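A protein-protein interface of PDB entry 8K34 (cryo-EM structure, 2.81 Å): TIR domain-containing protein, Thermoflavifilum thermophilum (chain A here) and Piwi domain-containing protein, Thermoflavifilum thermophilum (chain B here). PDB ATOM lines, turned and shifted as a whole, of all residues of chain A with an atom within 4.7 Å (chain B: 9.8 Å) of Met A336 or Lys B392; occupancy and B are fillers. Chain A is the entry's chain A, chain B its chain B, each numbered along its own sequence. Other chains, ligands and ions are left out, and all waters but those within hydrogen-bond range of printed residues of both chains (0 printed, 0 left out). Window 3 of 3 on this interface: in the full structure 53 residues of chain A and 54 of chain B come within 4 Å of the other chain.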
ATOM      1  N   ASN A 174      30.803  16.297 -22.326  1.00  0.00           N
ATOM      2  CA  ASN A 174      30.390  15.015 -21.772  1.00  0.00           C
ATOM      3  C   ASN A 174      29.147  14.496 -22.482  1.00  0.00           C
ATOM      4  O   ASN A 174      28.447  13.625 -21.957  1.00  0.00           O
ATOM      5  CB  ASN A 174      30.156  15.115 -20.264  1.00  0.00           C
ATOM      6  CG  ASN A 174      29.077  16.110 -19.903  1.00  0.00           C
ATOM      7  OD1 ASN A 174      28.607  16.869 -20.749  1.00  0.00           O
ATOM      8  ND2 ASN A 174      28.681  16.117 -18.637  1.00  0.00           N
ATOM      9  N   TRP A 175      28.862  15.031 -23.668  1.00  0.00           N
ATOM     10  CA  TRP A 175      27.694  14.671 -24.460  1.00  0.00           C
ATOM     11  C   TRP A 175      28.142  13.745 -25.581  1.00  0.00           C
ATOM     12  O   TRP A 175      28.768  14.187 -26.550  1.00  0.00           O
ATOM     13  CB  TRP A 175      27.024  15.920 -25.027  1.00  0.00           C
ATOM     14  CG  TRP A 175      26.110  16.593 -24.075  1.00  0.00           C
ATOM     15  CD1 TRP A 175      25.992  16.351 -22.740  1.00  0.00           C
ATOM     16  CD2 TRP A 175      25.183  17.634 -24.379  1.00  0.00           C
ATOM     17  NE1 TRP A 175      25.042  17.174 -22.195  1.00  0.00           N
ATOM     18  CE2 TRP A 175      24.529  17.973 -23.183  1.00  0.00           C
ATOM     19  CE3 TRP A 175      24.838  18.310 -25.553  1.00  0.00           C
ATOM     20  CZ2 TRP A 175      23.553  18.960 -23.122  1.00  0.00           C
ATOM     21  CZ3 TRP A 175      23.870  19.288 -25.492  1.00  0.00           C
ATOM     22  CH2 TRP A 175      23.238  19.604 -24.286  1.00  0.00           C
ATOM     23  N   SER A 324      27.395   8.506 -13.753  1.00  0.00           N
ATOM     24  CA  SER A 324      25.976   8.286 -13.979  1.00  0.00           C
ATOM     25  C   SER A 324      25.636   8.823 -15.360  1.00  0.00           C
ATOM     26  O   SER A 324      26.368   9.638 -15.918  1.00  0.00           O
ATOM     27  CB  SER A 324      25.115   8.968 -12.912  1.00  0.00           C
ATOM     28  OG  SER A 324      24.779  10.287 -13.301  1.00  0.00           O
ATOM     29  N   ALA A 325      24.525   8.362 -15.922  1.00  0.00           N
ATOM     30  CA  ALA A 325      24.182   8.721 -17.289  1.00  0.00           C
ATOM     31  C   ALA A 325      22.735   9.177 -17.385  1.00  0.00           C
ATOM     32  O   ALA A 325      21.887   8.817 -16.566  1.00  0.00           O
ATOM     33  CB  ALA A 325      24.419   7.556 -18.253  1.00  0.00           C
ATOM     34  N   ALA A 326      22.474   9.984 -18.411  1.00  0.00           N
ATOM     35  CA  ALA A 326      21.127  10.465 -18.695  1.00  0.00           C
ATOM     36  C   ALA A 326      21.048  10.836 -20.167  1.00  0.00           C
ATOM     37  O   ALA A 326      21.875  11.607 -20.654  1.00  0.00           O
ATOM     38  CB  ALA A 326      20.775  11.669 -17.817  1.00  0.00           C
ATOM     39  N   GLY A 327      20.067  10.289 -20.870  1.00  0.00           N
ATOM     40  CA  GLY A 327      19.941  10.572 -22.281  1.00  0.00           C
ATOM     41  C   GLY A 327      19.261  11.898 -22.563  1.00  0.00           C
ATOM     42  O   GLY A 327      18.688  12.537 -21.683  1.00  0.00           O
ATOM     43  N   LYS A 328      19.349  12.317 -23.823  1.00  0.00           N
ATOM     44  CA  LYS A 328      18.588  13.449 -24.331  1.00  0.00           C
ATOM     45  C   LYS A 328      18.588  13.360 -25.846  1.00  0.00           C
ATOM     46  O   LYS A 328      19.450  12.705 -26.437  1.00  0.00           O
ATOM     47  CB  LYS A 328      19.164  14.790 -23.870  1.00  0.00           C
ATOM     48  CG  LYS A 328      20.038  15.491 -24.902  1.00  0.00           C
ATOM     49  CD  LYS A 328      20.342  16.933 -24.510  1.00  0.00           C
ATOM     50  CE  LYS A 328      19.114  17.650 -23.981  1.00  0.00           C
ATOM     51  NZ  LYS A 328      19.447  19.005 -23.465  1.00  0.00           N
ATOM     52  N   VAL A 334      22.006  12.696 -27.802  1.00  0.00           N
ATOM     53  CA  VAL A 334      23.244  12.498 -27.061  1.00  0.00           C
ATOM     54  C   VAL A 334      22.925  11.882 -25.704  1.00  0.00           C
ATOM     55  O   VAL A 334      21.767  11.719 -25.320  1.00  0.00           O
ATOM     56  CB  VAL A 334      24.042  13.810 -26.877  1.00  0.00           C
ATOM     57  CG1 VAL A 334      24.069  14.622 -28.163  1.00  0.00           C
ATOM     58  CG2 VAL A 334      23.455  14.635 -25.744  1.00  0.00           C
ATOM     59  N   LEU A 335      23.983  11.520 -24.989  1.00  0.00           N
ATOM     60  CA  LEU A 335      23.888  11.071 -23.608  1.00  0.00           C
ATOM     61  C   LEU A 335      24.893  11.862 -22.789  1.00  0.00           C
ATOM     62  O   LEU A 335      26.046  12.010 -23.204  1.00  0.00           O
ATOM     63  CB  LEU A 335      24.148   9.561 -23.505  1.00  0.00           C
ATOM     64  CG  LEU A 335      24.095   8.859 -22.145  1.00  0.00           C
ATOM     65  CD1 LEU A 335      23.717   7.406 -22.320  1.00  0.00           C
ATOM     66  CD2 LEU A 335      25.426   8.936 -21.440  1.00  0.00           C
ATOM     67  N   MET A 336      24.464  12.387 -21.642  1.00  0.00           N
ATOM     68  CA  MET A 336      25.371  13.068 -20.731  1.00  0.00           C
ATOM     69  C   MET A 336      25.792  12.114 -19.627  1.00  0.00           C
ATOM     70  O   MET A 336      24.975  11.356 -19.096  1.00  0.00           O
ATOM     71  CB  MET A 336      24.750  14.312 -20.093  1.00  0.00           C
ATOM     72  CG  MET A 336      23.311  14.174 -19.653  1.00  0.00           C
ATOM     73  SD  MET A 336      22.344  15.633 -20.064  1.00  0.00           S
ATOM     74  CE  MET A 336      21.780  15.185 -21.690  1.00  0.00           C
ATOM     75  N   VAL A 337      27.073  12.163 -19.282  1.00  0.00           N
ATOM     76  CA  VAL A 337      27.633  11.391 -18.185  1.00  0.00           C
ATOM     77  C   VAL A 337      28.105  12.368 -17.121  1.00  0.00           C
ATOM     78  O   VAL A 337      28.938  13.241 -17.396  1.00  0.00           O
ATOM     79  CB  VAL A 337      28.782  10.485 -18.648  1.00  0.00           C
ATOM     80  CG1 VAL A 337      29.645  10.101 -17.474  1.00  0.00           C
ATOM     81  CG2 VAL A 337      28.232   9.245 -19.310  1.00  0.00           C
ATOM     82  N   SER A 338      27.569  12.225 -15.919  1.00  0.00           N
ATOM     83  CA  SER A 338      27.976  13.013 -14.768  1.00  0.00           C
ATOM     84  C   SER A 338      29.020  12.232 -13.987  1.00  0.00           C
ATOM     85  O   SER A 338      28.856  11.030 -13.756  1.00  0.00           O
ATOM     86  CB  SER A 338      26.778  13.339 -13.876  1.00  0.00           C
ATOM     87  OG  SER A 338      25.641  13.666 -14.651  1.00  0.00           O
ATOM     88  N   ARG B 364      11.004  26.211 -14.529  1.00  0.00           N
ATOM     89  CA  ARG B 364      10.093  26.734 -15.535  1.00  0.00           C
ATOM     90  C   ARG B 364       8.727  26.996 -14.916  1.00  0.00           C
ATOM     91  O   ARG B 364       8.261  26.238 -14.062  1.00  0.00           O
ATOM     92  CB  ARG B 364       9.961  25.748 -16.694  1.00  0.00           C
ATOM     93  CG  ARG B 364      10.971  25.953 -17.802  1.00  0.00           C
ATOM     94  CD  ARG B 364      11.384  24.623 -18.406  1.00  0.00           C
ATOM     95  NE  ARG B 364      11.416  23.561 -17.408  1.00  0.00           N
ATOM     96  CZ  ARG B 364      11.006  22.318 -17.622  1.00  0.00           C
ATOM     97  NH1 ARG B 364      10.523  21.941 -18.794  1.00  0.00           N
ATOM     98  NH2 ARG B 364      11.084  21.430 -16.635  1.00  0.00           N
ATOM     99  N   THR B 389      19.185  27.266 -14.551  1.00  0.00           N
ATOM    100  CA  THR B 389      19.261  25.960 -13.913  1.00  0.00           C
ATOM    101  C   THR B 389      20.701  25.477 -13.834  1.00  0.00           C
ATOM    102  O   THR B 389      21.503  25.725 -14.739  1.00  0.00           O
ATOM    103  CB  THR B 389      18.423  24.932 -14.679  1.00  0.00           C
ATOM    104  OG1 THR B 389      18.511  25.197 -16.084  1.00  0.00           O
ATOM    105  CG2 THR B 389      16.972  25.003 -14.249  1.00  0.00           C
ATOM    106  N   LYS B 390      21.022  24.789 -12.738  1.00  0.00           N
ATOM    107  CA  LYS B 390      22.251  24.002 -12.637  1.00  0.00           C
ATOM    108  C   LYS B 390      21.919  22.548 -12.976  1.00  0.00           C
ATOM    109  O   LYS B 390      22.021  21.632 -12.159  1.00  0.00           O
ATOM    110  CB  LYS B 390      22.864  24.138 -11.251  1.00  0.00           C
ATOM    111  CG  LYS B 390      23.335  25.541 -10.914  1.00  0.00           C
ATOM    112  CD  LYS B 390      23.178  25.822  -9.432  1.00  0.00           C
ATOM    113  CE  LYS B 390      24.402  26.518  -8.867  1.00  0.00           C
ATOM    114  NZ  LYS B 390      24.868  25.878  -7.606  1.00  0.00           N
ATOM    115  N   SER B 391      21.515  22.356 -14.226  1.00  0.00           N
ATOM    116  CA  SER B 391      20.881  21.120 -14.665  1.00  0.00           C
ATOM    117  C   SER B 391      21.931  20.038 -14.897  1.00  0.00           C
ATOM    118  O   SER B 391      23.086  20.142 -14.476  1.00  0.00           O
ATOM    119  CB  SER B 391      20.047  21.376 -15.916  1.00  0.00           C
ATOM    120  OG  SER B 391      20.841  21.275 -17.085  1.00  0.00           O
ATOM    121  N   LYS B 392      21.512  18.967 -15.565  1.00  0.00           N
ATOM    122  CA  LYS B 392      22.399  17.847 -15.832  1.00  0.00           C
ATOM    123  C   LYS B 392      23.619  18.325 -16.615  1.00  0.00           C
ATOM    124  O   LYS B 392      23.497  19.193 -17.489  1.00  0.00           O
ATOM    125  CB  LYS B 392      21.656  16.754 -16.602  1.00  0.00           C
ATOM    126  CG  LYS B 392      20.597  16.032 -15.773  1.00  0.00           C
ATOM    127  CD  LYS B 392      19.388  15.631 -16.608  1.00  0.00           C
ATOM    128  CE  LYS B 392      18.554  16.841 -16.990  1.00  0.00           C
ATOM    129  NZ  LYS B 392      17.942  16.696 -18.339  1.00  0.00           N
ATOM    130  N   PRO B 393      24.802  17.790 -16.327  1.00  0.00           N
ATOM    131  CA  PRO B 393      26.039  18.452 -16.759  1.00  0.00           C
ATOM    132  C   PRO B 393      26.249  18.395 -18.265  1.00  0.00           C
ATOM    133  O   PRO B 393      26.312  17.320 -18.864  1.00  0.00           O
ATOM    134  CB  PRO B 393      27.133  17.673 -16.016  1.00  0.00           C
ATOM    135  CG  PRO B 393      26.434  16.972 -14.900  1.00  0.00           C
ATOM    136  CD  PRO B 393      25.062  16.674 -15.406  1.00  0.00           C
ATOM    137  N   LEU B 394      26.357  19.574 -18.873  1.00  0.00           N
ATOM    138  CA  LEU B 394      27.104  19.754 -20.113  1.00  0.00           C
ATOM    139  C   LEU B 394      28.405  20.423 -19.685  1.00  0.00           C
ATOM    140  O   LEU B 394      28.557  21.642 -19.743  1.00  0.00           O
ATOM    141  CB  LEU B 394      26.344  20.590 -21.151  1.00  0.00           C
ATOM    142  CG  LEU B 394      27.166  21.075 -22.354  1.00  0.00           C
ATOM    143  CD1 LEU B 394      27.632  19.905 -23.194  1.00  0.00           C
ATOM    144  CD2 LEU B 394      26.390  22.062 -23.201  1.00  0.00           C
ATOM    145  N   LYS B 395      29.345  19.610 -19.223  1.00  0.00           N
ATOM    146  CA  LYS B 395      30.614  20.105 -18.703  1.00  0.00           C
ATOM    147  C   LYS B 395      31.622  20.062 -19.840  1.00  0.00           C
ATOM    148  O   LYS B 395      32.206  19.016 -20.130  1.00  0.00           O
ATOM    149  CB  LYS B 395      31.070  19.286 -17.503  1.00  0.00           C
ATOM    150  CG  LYS B 395      30.303  19.605 -16.234  1.00  0.00           C
ATOM    151  CD  LYS B 395      31.001  19.059 -15.003  1.00  0.00           C
ATOM    152  CE  LYS B 395      31.446  17.628 -15.208  1.00  0.00           C
ATOM    153  NZ  LYS B 395      32.611  17.296 -14.347  1.00  0.00           N
ATOM    154  N   LEU B 396      31.811  21.200 -20.497  1.00  0.00           N
ATOM    155  CA  LEU B 396      32.797  21.288 -21.556  1.00  0.00           C
ATOM    156  C   LEU B 396      34.204  21.162 -20.987  1.00  0.00           C
ATOM    157  O   LEU B 396      34.488  21.592 -19.867  1.00  0.00           O
ATOM    158  CB  LEU B 396      32.658  22.608 -22.306  1.00  0.00           C
ATOM    159  CG  LEU B 396      31.870  22.520 -23.606  1.00  0.00           C
ATOM    160  CD1 LEU B 396      32.107  23.753 -24.442  1.00  0.00           C
ATOM    161  CD2 LEU B 396      32.281  21.281 -24.357  1.00  0.00           C
ATOM    162  N   TYR B 397      35.084  20.553 -21.773  1.00  0.00           N
ATOM    163  CA  TYR B 397      36.491  20.434 -21.426  1.00  0.00           C
ATOM    164  C   TYR B 397      37.334  20.925 -22.588  1.00  0.00           C
ATOM    165  O   TYR B 397      37.131  20.495 -23.728  1.00  0.00           O
ATOM    166  CB  TYR B 397      36.871  18.992 -21.089  1.00  0.00           C
ATOM    167  CG  TYR B 397      36.022  18.336 -20.031  1.00  0.00           C
ATOM    168  CD1 TYR B 397      36.278  18.544 -18.687  1.00  0.00           C
ATOM    169  CD2 TYR B 397      34.990  17.477 -20.375  1.00  0.00           C
ATOM    170  CE1 TYR B 397      35.516  17.938 -17.715  1.00  0.00           C
ATOM    171  CE2 TYR B 397      34.225  16.864 -19.410  1.00  0.00           C
ATOM    172  CZ  TYR B 397      34.492  17.099 -18.081  1.00  0.00           C
ATOM    173  OH  TYR B 397      33.730  16.491 -17.113  1.00  0.00           O
ATOM    174  N   LYS B 417      16.867  28.318 -25.882  1.00  0.00           N
ATOM    175  CA  LYS B 417      17.658  27.590 -24.897  1.00  0.00           C
ATOM    176  C   LYS B 417      19.133  27.802 -25.194  1.00  0.00           C
ATOM    177  O   LYS B 417      19.560  27.677 -26.347  1.00  0.00           O
ATOM    178  CB  LYS B 417      17.335  26.092 -24.903  1.00  0.00           C
ATOM    179  CG  LYS B 417      15.854  25.757 -24.911  1.00  0.00           C
ATOM    180  CD  LYS B 417      15.618  24.362 -25.469  1.00  0.00           C
ATOM    181  CE  LYS B 417      15.597  23.311 -24.372  1.00  0.00           C
ATOM    182  NZ  LYS B 417      14.395  23.432 -23.508  1.00  0.00           N
ATOM    183  N   PHE B 419      23.349  27.714 -23.128  1.00  0.00           N
ATOM    184  CA  PHE B 419      24.205  27.478 -21.979  1.00  0.00           C
ATOM    185  C   PHE B 419      25.090  28.695 -21.770  1.00  0.00           C
ATOM    186  O   PHE B 419      25.642  29.239 -22.729  1.00  0.00           O
ATOM    187  CB  PHE B 419      25.077  26.237 -22.176  1.00  0.00           C
ATOM    188  CG  PHE B 419      24.331  24.942 -22.070  1.00  0.00           C
ATOM    189  CD1 PHE B 419      23.541  24.493 -23.111  1.00  0.00           C
ATOM    190  CD2 PHE B 419      24.435  24.164 -20.932  1.00  0.00           C
ATOM    191  CE1 PHE B 419      22.862  23.299 -23.015  1.00  0.00           C
ATOM    192  CE2 PHE B 419      23.757  22.969 -20.831  1.00  0.00           C
ATOM    193  CZ  PHE B 419      22.971  22.535 -21.874  1.00  0.00           C
ATOM    194  N   TRP B 421      28.429  30.014 -19.589  1.00  0.00           N
ATOM    195  CA  TRP B 421      29.554  29.636 -18.739  1.00  0.00           C
ATOM    196  C   TRP B 421      29.931  30.851 -17.907  1.00  0.00           C
ATOM    197  O   TRP B 421      30.827  31.620 -18.254  1.00  0.00           O
ATOM    198  CB  TRP B 421      30.720  29.120 -19.573  1.00  0.00           C
ATOM    199  CG  TRP B 421      30.739  27.628 -19.673  1.00  0.00           C
ATOM    200  CD1 TRP B 421      31.323  26.757 -18.804  1.00  0.00           C
ATOM    201  CD2 TRP B 421      30.130  26.829 -20.692  1.00  0.00           C
ATOM    202  NE1 TRP B 421      31.122  25.465 -19.221  1.00  0.00           N
ATOM    203  CE2 TRP B 421      30.389  25.484 -20.378  1.00  0.00           C
ATOM    204  CE3 TRP B 421      29.391  27.123 -21.840  1.00  0.00           C
ATOM    205  CZ2 TRP B 421      29.938  24.436 -21.171  1.00  0.00           C
ATOM    206  CZ3 TRP B 421      28.944  26.083 -22.623  1.00  0.00           C
ATOM    207  CH2 TRP B 421      29.220  24.756 -22.288  1.00  0.00           C
ATOM    208  N   PRO B 438      33.819  24.184 -14.580  1.00  0.00           N
ATOM    209  CA  PRO B 438      32.651  25.067 -14.646  1.00  0.00           C
ATOM    210  C   PRO B 438      31.418  24.368 -15.184  1.00  0.00           C
ATOM    211  O   PRO B 438      31.333  24.060 -16.377  1.00  0.00           O
ATOM    212  CB  PRO B 438      33.112  26.185 -15.591  1.00  0.00           C
ATOM    213  CG  PRO B 438      34.175  25.560 -16.414  1.00  0.00           C
ATOM    214  CD  PRO B 438      34.888  24.624 -15.488  1.00  0.00           C
ATOM    215  N   ASN B 439      30.459  24.112 -14.308  1.00  0.00           N
ATOM    216  CA  ASN B 439      29.155  23.656 -14.750  1.00  0.00           C
ATOM    217  C   ASN B 439      28.367  24.860 -15.245  1.00  0.00           C
ATOM    218  O   ASN B 439      28.077  25.762 -14.452  1.00  0.00           O
ATOM    219  CB  ASN B 439      28.413  22.968 -13.613  1.00  0.00           C
ATOM    220  CG  ASN B 439      27.899  21.599 -13.998  1.00  0.00           C
ATOM    221  OD1 ASN B 439      27.537  21.361 -15.150  1.00  0.00           O
ATOM    222  ND2 ASN B 439      27.861  20.688 -13.033  1.00  0.00           N
ATOM    223  N   PRO B 440      28.012  24.923 -16.522  1.00  0.00           N
ATOM    224  CA  PRO B 440      27.315  26.104 -17.029  1.00  0.00           C
ATOM    225  C   PRO B 440      25.907  26.185 -16.471  1.00  0.00           C
ATOM    226  O   PRO B 440      25.302  25.188 -16.073  1.00  0.00           O
ATOM    227  CB  PRO B 440      27.296  25.888 -18.543  1.00  0.00           C
ATOM    228  CG  PRO B 440      27.356  24.423 -18.712  1.00  0.00           C
ATOM    229  CD  PRO B 440      28.071  23.843 -17.518  1.00  0.00           C
ATOM    230  N   ILE B 441      25.390  27.406 -16.432  1.00  0.00           N
ATOM    231  CA  ILE B 441      23.981  27.606 -16.127  1.00  0.00           C
ATOM    232  C   ILE B 441      23.196  27.426 -17.419  1.00  0.00           C
ATOM    233  O   ILE B 441      23.446  28.113 -18.417  1.00  0.00           O
ATOM    234  CB  ILE B 441      23.729  28.985 -15.501  1.00  0.00           C
ATOM    235  CG1 ILE B 441      24.453  30.081 -16.281  1.00  0.00           C
ATOM    236  CG2 ILE B 441      24.172  28.997 -14.049  1.00  0.00           C
ATOM    237  CD1 ILE B 441      23.830  31.441 -16.119  1.00  0.00           C
ATOM    238  N   PHE B 442      22.281  26.466 -17.421  1.00  0.00           N
ATOM    239  CA  PHE B 442      21.369  26.312 -18.541  1.00  0.00           C
ATOM    240  C   PHE B 442      20.297  27.381 -18.413  1.00  0.00           C
ATOM    241  O   PHE B 442      19.546  27.399 -17.431  1.00  0.00           O
ATOM    242  CB  PHE B 442      20.754  24.915 -18.560  1.00  0.00           C
ATOM    243  CG  PHE B 442      19.892  24.653 -19.760  1.00  0.00           C
ATOM    244  CD1 PHE B 442      20.220  25.194 -20.989  1.00  0.00           C
ATOM    245  CD2 PHE B 442      18.754  23.877 -19.659  1.00  0.00           C
ATOM    246  CE1 PHE B 442      19.432  24.967 -22.096  1.00  0.00           C
ATOM    247  CE2 PHE B 442      17.962  23.645 -20.764  1.00  0.00           C
ATOM    248  CZ  PHE B 442      18.303  24.192 -21.984  1.00  0.00           C
ATOM    249  N   GLU B 444      16.999  29.179 -20.148  1.00  0.00           N
ATOM    250  CA  GLU B 444      15.933  28.817 -21.070  1.00  0.00           C
ATOM    251  C   GLU B 444      14.908  29.937 -21.111  1.00  0.00           C
ATOM    252  O   GLU B 444      14.399  30.351 -20.066  1.00  0.00           O
ATOM    253  CB  GLU B 444      15.274  27.502 -20.656  1.00  0.00           C
ATOM    254  CG  GLU B 444      14.362  26.904 -21.709  1.00  0.00           C
ATOM    255  CD  GLU B 444      13.814  25.555 -21.301  1.00  0.00           C
ATOM    256  OE1 GLU B 444      14.155  25.085 -20.196  1.00  0.00           O
ATOM    257  OE2 GLU B 444      13.043  24.962 -22.083  1.00  0.00           O
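Asn A174 touches Leu B394 (OD1 to CA, 3.3 Å).
Trp A175 touches Pro B393 (NE1 to O, 3.6 Å).
CD2 of Trp A175 touches CD1 of Leu B394 (3.5 Å).
Phe B419 touches Trp A175.
Lys B392 touches Met A336.
Met A336 touches Pro B393.
Pro B393 touches Ser A338 (CD to OG, 3.2 Å).
O of Val A337 is in hydrogen-bond range of ND2 of Asn A174.
O of Ser A324 is in hydrogen-bond range of N of Ser A338, at 2.9 Å.
N of Met A336 is in hydrogen-bond range of O of Ala A326 (2.9 Å).
The indole nitrogen (NE1) of Trp A175 sits close to the side-chain sulfur (SD) of Met A336, at 3.8 Å.
The side-chain amino group of Lys B395 is in hydrogen-bond range of the side-chain hydroxyl of Tyr B397 (3.1 Å).
No residue of chain B comes within 4 Å of Gly A327.
Lys A328 touches none of the printed residues of chain B.
No residue of chain B comes within 4 Å of Leu A335.
Met A336 touches just these residues of chain B: Lys B392 and Pro B393.
No residue of chain B comes within 4 Å of Val A337.
Ser B391 touches none of the printed residues of chain A.
Lys B392 touches one residue of chain A.
Of the printed residues of chain A, Pro B393 touches Asn A174 (2.7 Å), Trp A175 (3.6 Å), Met A336 (3.6 Å) and Ser A338 (3.2 Å).
Of the printed residues of chain A, Lys B395 touches Asn A174 (3.2 Å).
Of the 12 printed residues of chain A, 4 touch a printed residue of chain B.
Hydrophobic or aromatic side chains of chain A within 4 Å of the printed part of chain B: Trp A175 and Met A336.
Along chain A the printed residues that touch a printed residue of chain B span positions 174 to 338.
Printed residues of chain B that touch a printed residue of chain A: Lys B392, Pro B393, Leu B394, Lys B395 and Phe B419.
Among the printed residues, no Asp or Glu carboxylate lies within 4 Å of a Lys or Arg side-chain nitrogen of the other chain.
OD1 of Asn A174 lies within hydrogen-bond range of N of Lys B395.
O of Pro B393 sits at hydrogen-bond distance from ND2 of Asn A174.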
